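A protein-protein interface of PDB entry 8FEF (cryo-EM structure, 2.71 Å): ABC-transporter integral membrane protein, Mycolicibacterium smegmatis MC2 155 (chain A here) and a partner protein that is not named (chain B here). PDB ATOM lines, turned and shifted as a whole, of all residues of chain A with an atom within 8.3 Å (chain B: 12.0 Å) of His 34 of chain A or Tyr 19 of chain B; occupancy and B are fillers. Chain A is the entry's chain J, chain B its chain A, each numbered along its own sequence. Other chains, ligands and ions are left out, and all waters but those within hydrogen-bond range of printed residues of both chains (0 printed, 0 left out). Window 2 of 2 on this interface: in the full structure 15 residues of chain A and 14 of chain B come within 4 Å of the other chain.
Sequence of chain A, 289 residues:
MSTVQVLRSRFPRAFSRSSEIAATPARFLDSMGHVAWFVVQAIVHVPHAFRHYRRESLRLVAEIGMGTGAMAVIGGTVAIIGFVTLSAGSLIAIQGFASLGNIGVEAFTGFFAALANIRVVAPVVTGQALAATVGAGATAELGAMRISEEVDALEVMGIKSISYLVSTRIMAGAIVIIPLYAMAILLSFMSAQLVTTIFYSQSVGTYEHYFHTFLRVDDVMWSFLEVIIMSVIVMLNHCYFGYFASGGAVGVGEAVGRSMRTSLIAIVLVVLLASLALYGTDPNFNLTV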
ATOM      1  N   ARG A  27     -27.653  18.496   6.632  1.00  0.00           N
ATOM      2  CA  ARG A  27     -27.289  18.341   8.036  1.00  0.00           C
ATOM      3  C   ARG A  27     -25.847  17.869   8.182  1.00  0.00           C
ATOM      4  O   ARG A  27     -24.947  18.672   8.432  1.00  0.00           O
ATOM      5  CB  ARG A  27     -28.236  17.360   8.729  1.00  0.00           C
ATOM      6  CG  ARG A  27     -29.540  17.986   9.190  1.00  0.00           C
ATOM      7  CD  ARG A  27     -29.280  19.097  10.195  1.00  0.00           C
ATOM      8  NE  ARG A  27     -28.458  18.638  11.309  1.00  0.00           N
ATOM      9  CZ  ARG A  27     -28.042  19.411  12.302  1.00  0.00           C
ATOM     10  NH1 ARG A  27     -28.353  20.696  12.355  1.00  0.00           N
ATOM     11  NH2 ARG A  27     -27.294  18.882  13.266  1.00  0.00           N
ATOM     12  N   PHE A  28     -25.642  16.558   8.041  1.00  0.00           N
ATOM     13  CA  PHE A  28     -24.295  15.999   8.117  1.00  0.00           C
ATOM     14  C   PHE A  28     -23.412  16.557   7.007  1.00  0.00           C
ATOM     15  O   PHE A  28     -22.291  17.019   7.258  1.00  0.00           O
ATOM     16  CB  PHE A  28     -24.366  14.472   8.046  1.00  0.00           C
ATOM     17  CG  PHE A  28     -23.025  13.799   8.019  1.00  0.00           C
ATOM     18  CD1 PHE A  28     -22.264  13.695   9.171  1.00  0.00           C
ATOM     19  CD2 PHE A  28     -22.535  13.255   6.845  1.00  0.00           C
ATOM     20  CE1 PHE A  28     -21.031  13.069   9.149  1.00  0.00           C
ATOM     21  CE2 PHE A  28     -21.304  12.627   6.815  1.00  0.00           C
ATOM     22  CZ  PHE A  28     -20.550  12.535   7.969  1.00  0.00           C
ATOM     23  N   LEU A  29     -23.915  16.537   5.771  1.00  0.00           N
ATOM     24  CA  LEU A  29     -23.195  17.159   4.667  1.00  0.00           C
ATOM     25  C   LEU A  29     -23.051  18.658   4.887  1.00  0.00           C
ATOM     26  O   LEU A  29     -22.022  19.247   4.544  1.00  0.00           O
ATOM     27  CB  LEU A  29     -23.906  16.871   3.344  1.00  0.00           C
ATOM     28  CG  LEU A  29     -23.271  17.458   2.081  1.00  0.00           C
ATOM     29  CD1 LEU A  29     -21.876  16.892   1.867  1.00  0.00           C
ATOM     30  CD2 LEU A  29     -24.149  17.203   0.867  1.00  0.00           C
ATOM     31  N   ASP A  30     -24.072  19.293   5.471  1.00  0.00           N
ATOM     32  CA  ASP A  30     -23.995  20.724   5.746  1.00  0.00           C
ATOM     33  C   ASP A  30     -22.926  21.033   6.790  1.00  0.00           C
ATOM     34  O   ASP A  30     -22.186  22.012   6.656  1.00  0.00           O
ATOM     35  CB  ASP A  30     -25.359  21.243   6.201  1.00  0.00           C
ATOM     36  CG  ASP A  30     -25.513  22.736   5.990  1.00  0.00           C
ATOM     37  OD1 ASP A  30     -24.639  23.339   5.332  1.00  0.00           O
ATOM     38  OD2 ASP A  30     -26.509  23.308   6.482  1.00  0.00           O
ATOM     39  N   SER A  31     -22.835  20.211   7.840  1.00  0.00           N
ATOM     40  CA  SER A  31     -21.800  20.409   8.851  1.00  0.00           C
ATOM     41  C   SER A  31     -20.408  20.183   8.272  1.00  0.00           C
ATOM     42  O   SER A  31     -19.470  20.940   8.571  1.00  0.00           O
ATOM     43  CB  SER A  31     -22.044  19.481  10.040  1.00  0.00           C
ATOM     44  OG  SER A  31     -21.060  19.668  11.042  1.00  0.00           O
ATOM     45  N   MET A  32     -20.252  19.139   7.451  1.00  0.00           N
ATOM     46  CA  MET A  32     -18.973  18.913   6.786  1.00  0.00           C
ATOM     47  C   MET A  32     -18.614  20.080   5.877  1.00  0.00           C
ATOM     48  O   MET A  32     -17.451  20.488   5.806  1.00  0.00           O
ATOM     49  CB  MET A  32     -19.005  17.608   5.992  1.00  0.00           C
ATOM     50  CG  MET A  32     -19.139  16.360   6.842  1.00  0.00           C
ATOM     51  SD  MET A  32     -18.779  14.863   5.903  1.00  0.00           S
ATOM     52  CE  MET A  32     -17.040  15.096   5.545  1.00  0.00           C
ATOM     53  N   GLY A  33     -19.602  20.635   5.176  1.00  0.00           N
ATOM     54  CA  GLY A  33     -19.336  21.791   4.340  1.00  0.00           C
ATOM     55  C   GLY A  33     -18.963  23.024   5.137  1.00  0.00           C
ATOM     56  O   GLY A  33     -18.115  23.810   4.713  1.00  0.00           O
ATOM     57  N   HIS A  34     -19.591  23.213   6.299  1.00  0.00           N
ATOM     58  CA  HIS A  34     -19.247  24.349   7.149  1.00  0.00           C
ATOM     59  C   HIS A  34     -17.816  24.240   7.663  1.00  0.00           C
ATOM     60  O   HIS A  34     -17.053  25.217   7.624  1.00  0.00           O
ATOM     61  CB  HIS A  34     -20.235  24.449   8.311  1.00  0.00           C
ATOM     62  CG  HIS A  34     -20.128  25.724   9.086  1.00  0.00           C
ATOM     63  ND1 HIS A  34     -20.225  26.965   8.494  1.00  0.00           N
ATOM     64  CD2 HIS A  34     -19.938  25.951  10.407  1.00  0.00           C
ATOM     65  CE1 HIS A  34     -20.095  27.901   9.417  1.00  0.00           C
ATOM     66  NE2 HIS A  34     -19.921  27.313  10.586  1.00  0.00           N
ATOM     67  N   VAL A  35     -17.423  23.054   8.135  1.00  0.00           N
ATOM     68  CA  VAL A  35     -16.051  22.902   8.617  1.00  0.00           C
ATOM     69  C   VAL A  35     -15.056  22.985   7.459  1.00  0.00           C
ATOM     70  O   VAL A  35     -13.949  23.519   7.623  1.00  0.00           O
ATOM     71  CB  VAL A  35     -15.888  21.609   9.448  1.00  0.00           C
ATOM     72  CG1 VAL A  35     -16.074  20.363   8.608  1.00  0.00           C
ATOM     73  CG2 VAL A  35     -14.535  21.589  10.146  1.00  0.00           C
ATOM     74  N   ALA A  36     -15.425  22.487   6.274  1.00  0.00           N
ATOM     75  CA  ALA A  36     -14.556  22.614   5.110  1.00  0.00           C
ATOM     76  C   ALA A  36     -14.376  24.072   4.707  1.00  0.00           C
ATOM     77  O   ALA A  36     -13.265  24.498   4.372  1.00  0.00           O
ATOM     78  CB  ALA A  36     -15.117  21.800   3.945  1.00  0.00           C
ATOM     79  N   TRP A  37     -15.457  24.853   4.735  1.00  0.00           N
ATOM     80  CA  TRP A  37     -15.345  26.277   4.446  1.00  0.00           C
ATOM     81  C   TRP A  37     -14.466  26.975   5.472  1.00  0.00           C
ATOM     82  O   TRP A  37     -13.651  27.833   5.116  1.00  0.00           O
ATOM     83  CB  TRP A  37     -16.730  26.923   4.404  1.00  0.00           C
ATOM     84  CG  TRP A  37     -16.679  28.418   4.286  1.00  0.00           C
ATOM     85  CD1 TRP A  37     -16.605  29.147   3.135  1.00  0.00           C
ATOM     86  CD2 TRP A  37     -16.695  29.368   5.359  1.00  0.00           C
ATOM     87  NE1 TRP A  37     -16.573  30.489   3.424  1.00  0.00           N
ATOM     88  CE2 TRP A  37     -16.627  30.652   4.783  1.00  0.00           C
ATOM     89  CE3 TRP A  37     -16.760  29.257   6.752  1.00  0.00           C
ATOM     90  CZ2 TRP A  37     -16.624  31.814   5.549  1.00  0.00           C
ATOM     91  CZ3 TRP A  37     -16.755  30.412   7.511  1.00  0.00           C
ATOM     92  CH2 TRP A  37     -16.688  31.673   6.909  1.00  0.00           C
ATOM     93  N   PHE A  38     -14.620  26.621   6.750  1.00  0.00           N
ATOM     94  CA  PHE A  38     -13.791  27.225   7.789  1.00  0.00           C
ATOM     95  C   PHE A  38     -12.312  26.926   7.568  1.00  0.00           C
ATOM     96  O   PHE A  38     -11.469  27.825   7.652  1.00  0.00           O
ATOM     97  CB  PHE A  38     -14.235  26.742   9.170  1.00  0.00           C
ATOM     98  CG  PHE A  38     -13.394  27.280  10.295  1.00  0.00           C
ATOM     99  CD1 PHE A  38     -13.621  28.547  10.801  1.00  0.00           C
ATOM    100  CD2 PHE A  38     -12.376  26.519  10.845  1.00  0.00           C
ATOM    101  CE1 PHE A  38     -12.851  29.043  11.830  1.00  0.00           C
ATOM    102  CE2 PHE A  38     -11.601  27.014  11.868  1.00  0.00           C
ATOM    103  CZ  PHE A  38     -11.843  28.276  12.364  1.00  0.00           C
ATOM    104  N   VAL A  39     -11.975  25.665   7.278  1.00  0.00           N
ATOM    105  CA  VAL A  39     -10.564  25.319   7.117  1.00  0.00           C
ATOM    106  C   VAL A  39      -9.994  25.941   5.844  1.00  0.00           C
ATOM    107  O   VAL A  39      -8.846  26.400   5.831  1.00  0.00           O
ATOM    108  CB  VAL A  39     -10.346  23.792   7.176  1.00  0.00           C
ATOM    109  CG1 VAL A  39     -10.806  23.245   8.519  1.00  0.00           C
ATOM    110  CG2 VAL A  39     -11.037  23.070   6.042  1.00  0.00           C
ATOM    111  N   VAL A  40     -10.782  25.989   4.765  1.00  0.00           N
ATOM    112  CA  VAL A  40     -10.315  26.623   3.534  1.00  0.00           C
ATOM    113  C   VAL A  40     -10.066  28.109   3.763  1.00  0.00           C
ATOM    114  O   VAL A  40      -9.032  28.652   3.355  1.00  0.00           O
ATOM    115  CB  VAL A  40     -11.317  26.386   2.389  1.00  0.00           C
ATOM    116  CG1 VAL A  40     -11.030  27.317   1.224  1.00  0.00           C
ATOM    117  CG2 VAL A  40     -11.251  24.941   1.924  1.00  0.00           C
ATOM    118  N   GLN A  41     -11.001  28.784   4.437  1.00  0.00           N
ATOM    119  CA  GLN A  41     -10.850  30.211   4.699  1.00  0.00           C
ATOM    120  C   GLN A  41      -9.666  30.488   5.615  1.00  0.00           C
ATOM    121  O   GLN A  41      -8.969  31.495   5.449  1.00  0.00           O
ATOM    122  CB  GLN A  41     -12.137  30.769   5.304  1.00  0.00           C
ATOM    123  CG  GLN A  41     -12.245  32.283   5.261  1.00  0.00           C
ATOM    124  CD  GLN A  41     -12.508  32.814   3.864  1.00  0.00           C
ATOM    125  OE1 GLN A  41     -12.859  32.061   2.955  1.00  0.00           O
ATOM    126  NE2 GLN A  41     -12.339  34.119   3.687  1.00  0.00           N
ATOM    127  N   ILE A 162     -11.524  35.764  10.789  1.00  0.00           N
ATOM    128  CA  ILE A 162     -10.842  34.486  10.606  1.00  0.00           C
ATOM    129  C   ILE A 162      -9.359  34.710  10.344  1.00  0.00           C
ATOM    130  O   ILE A 162      -8.506  34.070  10.963  1.00  0.00           O
ATOM    131  CB  ILE A 162     -11.504  33.675   9.479  1.00  0.00           C
ATOM    132  CG1 ILE A 162     -12.851  33.124   9.950  1.00  0.00           C
ATOM    133  CG2 ILE A 162     -10.597  32.543   9.033  1.00  0.00           C
ATOM    134  CD1 ILE A 162     -13.476  32.125   9.004  1.00  0.00           C
ATOM    135  N   TYR A 240     -11.911  25.927  15.154  1.00  0.00           N
ATOM    136  CA  TYR A 240     -13.296  25.808  14.709  1.00  0.00           C
ATOM    137  C   TYR A 240     -14.249  25.701  15.887  1.00  0.00           C
ATOM    138  O   TYR A 240     -15.307  26.342  15.899  1.00  0.00           O
ATOM    139  CB  TYR A 240     -13.460  24.601  13.788  1.00  0.00           C
ATOM    140  CG  TYR A 240     -14.904  24.296  13.458  1.00  0.00           C
ATOM    141  CD1 TYR A 240     -15.578  25.020  12.485  1.00  0.00           C
ATOM    142  CD2 TYR A 240     -15.592  23.284  14.114  1.00  0.00           C
ATOM    143  CE1 TYR A 240     -16.895  24.752  12.180  1.00  0.00           C
ATOM    144  CE2 TYR A 240     -16.911  23.009  13.816  1.00  0.00           C
ATOM    145  CZ  TYR A 240     -17.556  23.745  12.846  1.00  0.00           C
ATOM    146  OH  TYR A 240     -18.869  23.473  12.543  1.00  0.00           O
ATOM    147  N   TYR A 243     -14.304  29.151  17.713  1.00  0.00           N
ATOM    148  CA  TYR A 243     -14.712  30.321  16.943  1.00  0.00           C
ATOM    149  C   TYR A 243     -16.228  30.422  16.845  1.00  0.00           C
ATOM    150  O   TYR A 243     -16.784  31.525  16.878  1.00  0.00           O
ATOM    151  CB  TYR A 243     -14.078  30.267  15.553  1.00  0.00           C
ATOM    152  CG  TYR A 243     -14.311  31.494  14.700  1.00  0.00           C
ATOM    153  CD1 TYR A 243     -13.523  32.627  14.849  1.00  0.00           C
ATOM    154  CD2 TYR A 243     -15.306  31.512  13.735  1.00  0.00           C
ATOM    155  CE1 TYR A 243     -13.729  33.746  14.070  1.00  0.00           C
ATOM    156  CE2 TYR A 243     -15.519  32.625  12.951  1.00  0.00           C
ATOM    157  CZ  TYR A 243     -14.729  33.738  13.121  1.00  0.00           C
ATOM    158  OH  TYR A 243     -14.943  34.848  12.338  1.00  0.00           O
ATOM    159  N   PHE A 244     -16.912  29.287  16.725  1.00  0.00           N
ATOM    160  CA  PHE A 244     -18.367  29.250  16.598  1.00  0.00           C
ATOM    161  C   PHE A 244     -19.041  28.819  17.893  1.00  0.00           C
ATOM    162  O   PHE A 244     -20.049  28.109  17.871  1.00  0.00           O
ATOM    163  CB  PHE A 244     -18.772  28.333  15.451  1.00  0.00           C
ATOM    164  CG  PHE A 244     -18.268  28.783  14.110  1.00  0.00           C
ATOM    165  CD1 PHE A 244     -18.825  29.881  13.479  1.00  0.00           C
ATOM    166  CD2 PHE A 244     -17.240  28.104  13.479  1.00  0.00           C
ATOM    167  CE1 PHE A 244     -18.363  30.297  12.248  1.00  0.00           C
ATOM    168  CE2 PHE A 244     -16.778  28.514  12.247  1.00  0.00           C
ATOM    169  CZ  PHE A 244     -17.339  29.612  11.631  1.00  0.00           C
ATOM    170  N   PRO B  18     -21.267  28.339  -0.391  1.00  0.00           N
ATOM    171  CA  PRO B  18     -20.794  27.144  -1.098  1.00  0.00           C
ATOM    172  C   PRO B  18     -20.464  26.007  -0.139  1.00  0.00           C
ATOM    173  O   PRO B  18     -19.471  25.304  -0.331  1.00  0.00           O
ATOM    174  CB  PRO B  18     -19.536  27.640  -1.808  1.00  0.00           C
ATOM    175  CG  PRO B  18     -19.019  28.712  -0.912  1.00  0.00           C
ATOM    176  CD  PRO B  18     -20.235  29.389  -0.334  1.00  0.00           C
ATOM    177  N   TYR B  19     -21.296  25.842   0.892  1.00  0.00           N
ATOM    178  CA  TYR B  19     -21.037  24.823   1.904  1.00  0.00           C
ATOM    179  C   TYR B  19     -21.159  23.414   1.333  1.00  0.00           C
ATOM    180  O   TYR B  19     -20.256  22.589   1.510  1.00  0.00           O
ATOM    181  CB  TYR B  19     -21.982  25.009   3.093  1.00  0.00           C
ATOM    182  CG  TYR B  19     -21.738  26.281   3.875  1.00  0.00           C
ATOM    183  CD1 TYR B  19     -20.487  26.886   3.882  1.00  0.00           C
ATOM    184  CD2 TYR B  19     -22.754  26.870   4.615  1.00  0.00           C
ATOM    185  CE1 TYR B  19     -20.256  28.045   4.597  1.00  0.00           C
ATOM    186  CE2 TYR B  19     -22.534  28.031   5.334  1.00  0.00           C
ATOM    187  CZ  TYR B  19     -21.283  28.613   5.321  1.00  0.00           C
ATOM    188  OH  TYR B  19     -21.058  29.767   6.036  1.00  0.00           O
ATOM    189  N   LYS B  20     -22.263  23.119   0.643  1.00  0.00           N
ATOM    190  CA  LYS B  20     -22.475  21.764   0.141  1.00  0.00           C
ATOM    191  C   LYS B  20     -21.417  21.349  -0.875  1.00  0.00           C
ATOM    192  O   LYS B  20     -21.063  20.167  -0.950  1.00  0.00           O
ATOM    193  CB  LYS B  20     -23.874  21.646  -0.464  1.00  0.00           C
ATOM    194  CG  LYS B  20     -24.979  22.155   0.448  1.00  0.00           C
ATOM    195  CD  LYS B  20     -26.346  21.687  -0.019  1.00  0.00           C
ATOM    196  CE  LYS B  20     -26.489  20.182   0.134  1.00  0.00           C
ATOM    197  NZ  LYS B  20     -26.311  19.753   1.549  1.00  0.00           N
ATOM    198  N   LEU B  21     -20.909  22.294  -1.670  1.00  0.00           N
ATOM    199  CA  LEU B  21     -19.803  21.982  -2.573  1.00  0.00           C
ATOM    200  C   LEU B  21     -18.536  21.637  -1.796  1.00  0.00           C
ATOM    201  O   LEU B  21     -17.834  20.667  -2.125  1.00  0.00           O
ATOM    202  CB  LEU B  21     -19.552  23.157  -3.516  1.00  0.00           C
ATOM    203  CG  LEU B  21     -18.373  23.021  -4.482  1.00  0.00           C
ATOM    204  CD1 LEU B  21     -18.597  21.861  -5.441  1.00  0.00           C
ATOM    205  CD2 LEU B  21     -18.149  24.319  -5.243  1.00  0.00           C
ATOM    206  N   ALA B  22     -18.252  22.390  -0.730  1.00  0.00           N
ATOM    207  CA  ALA B  22     -17.012  22.157  -0.006  1.00  0.00           C
ATOM    208  C   ALA B  22     -17.088  20.885   0.822  1.00  0.00           C
ATOM    209  O   ALA B  22     -16.055  20.265   1.085  1.00  0.00           O
ATOM    210  CB  ALA B  22     -16.683  23.357   0.880  1.00  0.00           C
ATOM    211  N   GLY B  23     -18.287  20.491   1.258  1.00  0.00           N
ATOM    212  CA  GLY B  23     -18.403  19.232   1.973  1.00  0.00           C
ATOM    213  C   GLY B  23     -18.048  18.059   1.083  1.00  0.00           C
ATOM    214  O   GLY B  23     -17.347  17.131   1.501  1.00  0.00           O
ATOM    215  N   LEU B  24     -18.522  18.095  -0.167  1.00  0.00           N
ATOM    216  CA  LEU B  24     -18.166  17.074  -1.145  1.00  0.00           C
ATOM    217  C   LEU B  24     -16.673  17.089  -1.435  1.00  0.00           C
ATOM    218  O   LEU B  24     -16.048  16.030  -1.561  1.00  0.00           O
ATOM    219  CB  LEU B  24     -18.965  17.273  -2.432  1.00  0.00           C
ATOM    220  CG  LEU B  24     -20.487  17.163  -2.321  1.00  0.00           C
ATOM    221  CD1 LEU B  24     -21.138  17.331  -3.685  1.00  0.00           C
ATOM    222  CD2 LEU B  24     -20.885  15.836  -1.692  1.00  0.00           C
ATOM    223  N   ILE B  25     -16.084  18.285  -1.539  1.00  0.00           N
ATOM    224  CA  ILE B  25     -14.644  18.376  -1.778  1.00  0.00           C
ATOM    225  C   ILE B  25     -13.860  17.785  -0.610  1.00  0.00           C
ATOM    226  O   ILE B  25     -12.889  17.044  -0.808  1.00  0.00           O
ATOM    227  CB  ILE B  25     -14.239  19.836  -2.056  1.00  0.00           C
ATOM    228  CG1 ILE B  25     -14.877  20.327  -3.357  1.00  0.00           C
ATOM    229  CG2 ILE B  25     -12.725  19.974  -2.123  1.00  0.00           C
ATOM    230  CD1 ILE B  25     -14.476  21.733  -3.744  1.00  0.00           C
ATOM    231  N   LEU B  26     -14.273  18.093   0.623  1.00  0.00           N
ATOM    232  CA  LEU B  26     -13.605  17.549   1.803  1.00  0.00           C
ATOM    233  C   LEU B  26     -13.723  16.030   1.858  1.00  0.00           C
ATOM    234  O   LEU B  26     -12.743  15.333   2.154  1.00  0.00           O
ATOM    235  CB  LEU B  26     -14.185  18.177   3.070  1.00  0.00           C
ATOM    236  CG  LEU B  26     -13.596  17.701   4.399  1.00  0.00           C
ATOM    237  CD1 LEU B  26     -12.146  18.135   4.531  1.00  0.00           C
ATOM    238  CD2 LEU B  26     -14.419  18.208   5.571  1.00  0.00           C
ATOM    239  N   GLY B  27     -14.920  15.501   1.591  1.00  0.00           N
ATOM    240  CA  GLY B  27     -15.093  14.058   1.585  1.00  0.00           C
ATOM    241  C   GLY B  27     -14.260  13.377   0.516  1.00  0.00           C
ATOM    242  O   GLY B  27     -13.663  12.323   0.758  1.00  0.00           O
ATOM    243  N   LEU B  28     -14.199  13.974  -0.677  1.00  0.00           N
ATOM    244  CA  LEU B  28     -13.383  13.410  -1.747  1.00  0.00           C
ATOM    245  C   LEU B  28     -11.904  13.441  -1.383  1.00  0.00           C
ATOM    246  O   LEU B  28     -11.169  12.489  -1.670  1.00  0.00           O
ATOM    247  CB  LEU B  28     -13.633  14.168  -3.051  1.00  0.00           C
ATOM    248  CG  LEU B  28     -12.974  13.599  -4.308  1.00  0.00           C
ATOM    249  CD1 LEU B  28     -13.544  12.230  -4.637  1.00  0.00           C
ATOM    250  CD2 LEU B  28     -13.146  14.552  -5.479  1.00  0.00           C
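Of the 19 printed residues of chain A, 7 touch a printed residue of chain B. Printed residues of chain A that touch a printed residue of chain B: Leu 29, Asp 30, Met 32, Gly 33, His 34, Ala 36 and Trp 37. Hydrophobic or aromatic side chains of chain A that line the printed part of chain B: Leu 29, His 34, Ala 36 and Trp 37. Hydrophobic or aromatic side chains of chain B that line the printed part of chain A: Tyr 19, Ala 22, Leu 24 and Leu 26. Among the printed residues, 10 pairs touch across the chains.
Leu 29 of chain A touches Lys 20 of chain B. Leu 29 of chain A touches Leu 24 of chain B. Asp 30 of chain A touches Tyr 19 of chain B. Met 32 of chain A touches Leu 26 of chain B (O to CD2, 3.8 Å). Gly 33 of chain A touches Tyr 19 of chain B (CA to O, 3.1 Å). Gly 23 of chain B touches Gly 33 of chain A (N to CA, 3.5 Å). His 34 of chain A touches Tyr 19 of chain B. Ala 36 of chain A touches Ala 22 of chain B (CB to O, 3.4 Å). Ala 36 of chain A touches Leu 26 of chain B. CG of Trp 37 of chain A touches CE1 of Tyr 19 of chain B (3.6 Å).
Phe 28 of chain A touches none of the printed residues of chain B. Of the printed residues of chain B, Leu 29 of chain A touches Lys 20 and Leu 24. Of chain B, only Tyr 19 comes within 4 Å of Asp 30 of chain A. Ser 31 of chain A touches none of the printed residues of chain B. Gly 33 of chain A touches just these residues of chain B: Tyr 19 and Gly 23. His 34 of chain A touches just one residue of chain B: Tyr 19 (3.7 Å). No residue of chain B comes within 4 Å of Val 35 of chain A. Printed residues of chain B within 4 Å of Ala 36 of chain A: Ala 22 (3.4 Å) and Leu 26 (3.8 Å). Printed residues of chain B within 4 Å of Trp 37 of chain A: Tyr 19. No residue of chain A comes within 4 Å of Pro 18 of chain B. Tyr 19 of chain B touches just these residues of chain A: Asp 30, Gly 33, His 34 and Trp 37. Printed residues of chain A within 4 Å of Ala 22 of chain B: Ala 36. Of the printed residues of chain A, Gly 23 of chain B touches Gly 33 (3.5 Å). Printed residues of chain A within 4 Å of Leu 24 of chain B: Leu 29. Of the printed residues of chain A, Leu 26 of chain B touches Met 32 (3.8 Å) and Ala 36 (3.8 Å). The nearest residue of chain B that does not touch His 34 of chain A is Gly 23 of chain B (5.9 Å). The nearest printed residue of chain B that does not touch Met 32 of chain A is Gly 23 of chain B (4.001 Å).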
